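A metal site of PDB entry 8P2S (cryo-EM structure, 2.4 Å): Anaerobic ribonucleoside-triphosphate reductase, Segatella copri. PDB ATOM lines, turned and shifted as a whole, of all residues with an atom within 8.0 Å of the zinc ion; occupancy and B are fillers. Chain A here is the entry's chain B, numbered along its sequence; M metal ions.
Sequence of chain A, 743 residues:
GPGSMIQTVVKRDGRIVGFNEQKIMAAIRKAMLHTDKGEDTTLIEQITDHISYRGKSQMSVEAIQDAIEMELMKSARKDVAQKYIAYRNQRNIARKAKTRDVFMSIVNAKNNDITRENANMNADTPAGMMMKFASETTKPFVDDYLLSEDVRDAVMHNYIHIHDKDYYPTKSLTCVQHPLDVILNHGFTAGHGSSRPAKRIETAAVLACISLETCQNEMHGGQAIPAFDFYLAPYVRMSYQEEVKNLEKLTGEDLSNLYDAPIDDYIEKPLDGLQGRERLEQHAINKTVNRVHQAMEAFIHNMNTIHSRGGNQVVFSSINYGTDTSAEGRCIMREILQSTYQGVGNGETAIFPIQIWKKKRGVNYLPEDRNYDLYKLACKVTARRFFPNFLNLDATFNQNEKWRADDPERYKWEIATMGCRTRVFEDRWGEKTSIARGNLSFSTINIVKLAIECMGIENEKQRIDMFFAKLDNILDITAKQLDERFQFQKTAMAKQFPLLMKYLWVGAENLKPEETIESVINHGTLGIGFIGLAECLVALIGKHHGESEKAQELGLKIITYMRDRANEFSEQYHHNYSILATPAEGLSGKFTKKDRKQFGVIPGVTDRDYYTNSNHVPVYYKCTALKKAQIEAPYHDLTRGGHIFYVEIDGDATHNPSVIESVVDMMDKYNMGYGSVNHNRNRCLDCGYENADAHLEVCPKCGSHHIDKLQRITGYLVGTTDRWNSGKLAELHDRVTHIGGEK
The backbone NH (N) of Ser 704 lies close to the side-chain sulfur (SG) of Cys 702 (3.0 Å). N of Lys 701 lies close to SG of Cys 699 (3.4 Å). The backbone NH (N) of Asp 686 lies close to the side-chain sulfur (SG) of Cys 684 (3.5 Å). The backbone carbonyl oxygen (O) of Tyr 689 lies within hydrogen-bond range of the backbone NH (N) of Cys 684 (3.2 Å).
Within 4 Å of the zinc ion: Cys 684, Cys 687, Cys 699 and Cys 702.
The zinc ion is bound by the side-chain sulfur of Cys 702 (2.3 Å), the side-chain sulfur of Cys 687 (2.3 Å), the side-chain sulfur of Cys 699 (2.3 Å) and the side-chain sulfur of Cys 684 (2.3 Å). The zinc ion has four donor atoms within binding distance.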
ATOM      1  N   ARG A 683      -0.681   1.666  31.972  1.00  0.00           N
ATOM      2  CA  ARG A 683       0.266   2.525  31.278  1.00  0.00           C
ATOM      3  C   ARG A 683       1.675   1.939  31.337  1.00  0.00           C
ATOM      4  O   ARG A 683       2.120   1.477  32.390  1.00  0.00           O
ATOM      5  CB  ARG A 683       0.280   3.931  31.875  1.00  0.00           C
ATOM      6  CG  ARG A 683       1.350   4.840  31.281  1.00  0.00           C
ATOM      7  CD  ARG A 683       1.341   6.224  31.889  1.00  0.00           C
ATOM      8  NE  ARG A 683       1.237   6.182  33.340  1.00  0.00           N
ATOM      9  CZ  ARG A 683       0.131   6.512  34.012  1.00  0.00           C
ATOM     10  NH1 ARG A 683      -0.949   6.939  33.394  1.00  0.00           N
ATOM     11  NH2 ARG A 683       0.137   6.409  35.333  1.00  0.00           N
ATOM     12  N   CYS A 684       2.364   1.994  30.203  1.00  0.00           N
ATOM     13  CA  CYS A 684       3.775   1.637  30.134  1.00  0.00           C
ATOM     14  C   CYS A 684       4.612   2.808  30.634  1.00  0.00           C
ATOM     15  O   CYS A 684       4.526   3.911  30.081  1.00  0.00           O
ATOM     16  CB  CYS A 684       4.165   1.262  28.706  1.00  0.00           C
ATOM     17  SG  CYS A 684       5.943   1.133  28.403  1.00  0.00           S
ATOM     18  N   LEU A 685       5.409   2.571  31.671  1.00  0.00           N
ATOM     19  CA  LEU A 685       6.246   3.644  32.213  1.00  0.00           C
ATOM     20  C   LEU A 685       7.255   4.131  31.187  1.00  0.00           C
ATOM     21  O   LEU A 685       7.499   5.338  31.064  1.00  0.00           O
ATOM     22  CB  LEU A 685       6.950   3.166  33.483  1.00  0.00           C
ATOM     23  CG  LEU A 685       7.796   4.210  34.213  1.00  0.00           C
ATOM     24  CD1 LEU A 685       6.948   5.415  34.610  1.00  0.00           C
ATOM     25  CD2 LEU A 685       8.469   3.600  35.434  1.00  0.00           C
ATOM     26  N   ASP A 686       7.864   3.210  30.443  1.00  0.00           N
ATOM     27  CA  ASP A 686       8.847   3.593  29.432  1.00  0.00           C
ATOM     28  C   ASP A 686       8.194   4.354  28.284  1.00  0.00           C
ATOM     29  O   ASP A 686       8.742   5.342  27.791  1.00  0.00           O
ATOM     30  CB  ASP A 686       9.579   2.362  28.909  1.00  0.00           C
ATOM     31  CG  ASP A 686      10.613   2.696  27.861  1.00  0.00           C
ATOM     32  OD1 ASP A 686      11.650   3.306  28.213  1.00  0.00           O
ATOM     33  OD2 ASP A 686      10.400   2.357  26.682  1.00  0.00           O
ATOM     34  N   CYS A 687       7.017   3.900  27.838  1.00  0.00           N
ATOM     35  CA  CYS A 687       6.345   4.483  26.675  1.00  0.00           C
ATOM     36  C   CYS A 687       5.293   5.514  27.054  1.00  0.00           C
ATOM     37  O   CYS A 687       5.326   6.646  26.549  1.00  0.00           O
ATOM     38  CB  CYS A 687       5.683   3.372  25.843  1.00  0.00           C
ATOM     39  SG  CYS A 687       6.833   2.384  24.861  1.00  0.00           S
ATOM     40  N   GLY A 688       4.368   5.161  27.932  1.00  0.00           N
ATOM     41  CA  GLY A 688       3.199   5.982  28.193  1.00  0.00           C
ATOM     42  C   GLY A 688       1.929   5.504  27.535  1.00  0.00           C
ATOM     43  O   GLY A 688       0.893   6.168  27.667  1.00  0.00           O
ATOM     44  N   TYR A 689       1.983   4.387  26.810  1.00  0.00           N
ATOM     45  CA  TYR A 689       0.787   3.817  26.192  1.00  0.00           C
ATOM     46  C   TYR A 689      -0.188   3.353  27.260  1.00  0.00           C
ATOM     47  O   TYR A 689       0.090   2.413  27.998  1.00  0.00           O
ATOM     48  CB  TYR A 689       1.180   2.656  25.274  1.00  0.00           C
ATOM     49  CG  TYR A 689       0.000   1.890  24.723  1.00  0.00           C
ATOM     50  CD1 TYR A 689      -0.720   2.379  23.642  1.00  0.00           C
ATOM     51  CD2 TYR A 689      -0.385   0.671  25.262  1.00  0.00           C
ATOM     52  CE1 TYR A 689      -1.799   1.687  23.127  1.00  0.00           C
ATOM     53  CE2 TYR A 689      -1.458  -0.033  24.753  1.00  0.00           C
ATOM     54  CZ  TYR A 689      -2.160   0.477  23.684  1.00  0.00           C
ATOM     55  OH  TYR A 689      -3.236  -0.218  23.179  1.00  0.00           O
ATOM     56  N   VAL A 698       2.164  -6.407  29.389  1.00  0.00           N
ATOM     57  CA  VAL A 698       3.273  -5.797  28.657  1.00  0.00           C
ATOM     58  C   VAL A 698       2.724  -4.714  27.742  1.00  0.00           C
ATOM     59  O   VAL A 698       1.548  -4.686  27.400  1.00  0.00           O
ATOM     60  CB  VAL A 698       4.069  -6.835  27.847  1.00  0.00           C
ATOM     61  CG1 VAL A 698       4.744  -7.837  28.772  1.00  0.00           C
ATOM     62  CG2 VAL A 698       3.168  -7.542  26.848  1.00  0.00           C
ATOM     63  N   CYS A 699       3.623  -3.810  27.341  1.00  0.00           N
ATOM     64  CA  CYS A 699       3.252  -2.721  26.455  1.00  0.00           C
ATOM     65  C   CYS A 699       3.186  -3.220  25.016  1.00  0.00           C
ATOM     66  O   CYS A 699       4.185  -3.739  24.502  1.00  0.00           O
ATOM     67  CB  CYS A 699       4.263  -1.588  26.564  1.00  0.00           C
ATOM     68  SG  CYS A 699       3.963  -0.188  25.456  1.00  0.00           S
ATOM     69  N   PRO A 700       2.034  -3.100  24.341  1.00  0.00           N
ATOM     70  CA  PRO A 700       1.974  -3.506  22.924  1.00  0.00           C
ATOM     71  C   PRO A 700       2.923  -2.723  22.032  1.00  0.00           C
ATOM     72  O   PRO A 700       3.430  -3.275  21.047  1.00  0.00           O
ATOM     73  CB  PRO A 700       0.511  -3.251  22.556  1.00  0.00           C
ATOM     74  CG  PRO A 700      -0.228  -3.305  23.854  1.00  0.00           C
ATOM     75  CD  PRO A 700       0.717  -2.719  24.870  1.00  0.00           C
ATOM     76  N   LYS A 701       3.177  -1.447  22.348  1.00  0.00           N
ATOM     77  CA  LYS A 701       4.056  -0.640  21.513  1.00  0.00           C
ATOM     78  C   LYS A 701       5.500  -1.119  21.600  1.00  0.00           C
ATOM     79  O   LYS A 701       6.194  -1.228  20.582  1.00  0.00           O
ATOM     80  CB  LYS A 701       3.961   0.831  21.914  1.00  0.00           C
ATOM     81  CG  LYS A 701       2.615   1.473  21.595  1.00  0.00           C
ATOM     82  CD  LYS A 701       2.614   2.946  21.941  1.00  0.00           C
ATOM     83  CE  LYS A 701       3.704   3.696  21.190  1.00  0.00           C
ATOM     84  NZ  LYS A 701       3.537   3.597  19.713  1.00  0.00           N
ATOM     85  N   CYS A 702       5.975  -1.408  22.809  1.00  0.00           N
ATOM     86  CA  CYS A 702       7.372  -1.757  23.030  1.00  0.00           C
ATOM     87  C   CYS A 702       7.552  -3.178  23.564  1.00  0.00           C
ATOM     88  O   CYS A 702       8.380  -3.927  23.045  1.00  0.00           O
ATOM     89  CB  CYS A 702       8.030  -0.766  23.998  1.00  0.00           C
ATOM     90  SG  CYS A 702       7.632  -1.056  25.739  1.00  0.00           S
ATOM     91  N   GLY A 703       6.804  -3.546  24.588  1.00  0.00           N
ATOM     92  CA  GLY A 703       7.026  -4.816  25.255  1.00  0.00           C
ATOM     93  C   GLY A 703       7.768  -4.642  26.569  1.00  0.00           C
ATOM     94  O   GLY A 703       8.686  -5.394  26.884  1.00  0.00           O
ATOM     95  N   SER A 704       7.371  -3.628  27.342  1.00  0.00           N
ATOM     96  CA  SER A 704       8.025  -3.353  28.613  1.00  0.00           C
ATOM     97  C   SER A 704       7.788  -4.492  29.592  1.00  0.00           C
ATOM     98  O   SER A 704       6.836  -5.275  29.460  1.00  0.00           O
ATOM     99  CB  SER A 704       7.507  -2.036  29.205  1.00  0.00           C
ATOM    100  OG  SER A 704       8.221  -1.687  30.371  1.00  0.00           O
ATOM    101  N   HIS A 705       8.668  -4.588  30.586  1.00  0.00           N
ATOM    102  CA  HIS A 705       8.615  -5.684  31.540  1.00  0.00           C
ATOM    103  C   HIS A 705       7.298  -5.678  32.320  1.00  0.00           C
ATOM    104  O   HIS A 705       6.648  -6.722  32.468  1.00  0.00           O
ATOM    105  CB  HIS A 705       9.805  -5.602  32.503  1.00  0.00           C
ATOM    106  N   HIS A 706       6.886  -4.517  32.816  1.00  0.00           N
ATOM    107  CA  HIS A 706       5.682  -4.416  33.616  1.00  0.00           C
ATOM    108  C   HIS A 706       4.959  -3.123  33.303  1.00  0.00           C
ATOM    109  O   HIS A 706       5.560  -2.139  32.846  1.00  0.00           O
ATOM    110  CB  HIS A 706       5.995  -4.516  35.112  1.00  0.00           C
ATOM    111  CG  HIS A 706       6.271  -5.911  35.588  1.00  0.00           C
ATOM    112  ND1 HIS A 706       5.974  -7.022  34.843  1.00  0.00           N
ATOM    113  CD2 HIS A 706       6.833  -6.367  36.738  1.00  0.00           C
ATOM    114  CE1 HIS A 706       6.326  -8.110  35.499  1.00  0.00           C
ATOM    115  NE2 HIS A 706       6.858  -7.733  36.660  1.00  0.00           N
ATOM    116  N   ILE A 707       3.659  -3.123  33.569  1.00  0.00           N
ATOM    117  CA  ILE A 707       2.758  -2.020  33.235  1.00  0.00           C
ATOM    118  C   ILE A 707       2.138  -1.502  34.528  1.00  0.00           C
ATOM    119  O   ILE A 707       1.576  -2.297  35.303  1.00  0.00           O
ATOM    120  CB  ILE A 707       1.671  -2.459  32.245  1.00  0.00           C
ATOM    121  CG1 ILE A 707       2.315  -2.983  30.953  1.00  0.00           C
ATOM    122  CG2 ILE A 707       0.732  -1.321  31.938  1.00  0.00           C
ATOM    123  CD1 ILE A 707       3.104  -1.953  30.199  1.00  0.00           C
HETATM  124 ZN    ZN M   1       6.050   0.597  26.135  1.00  0.00          ZN
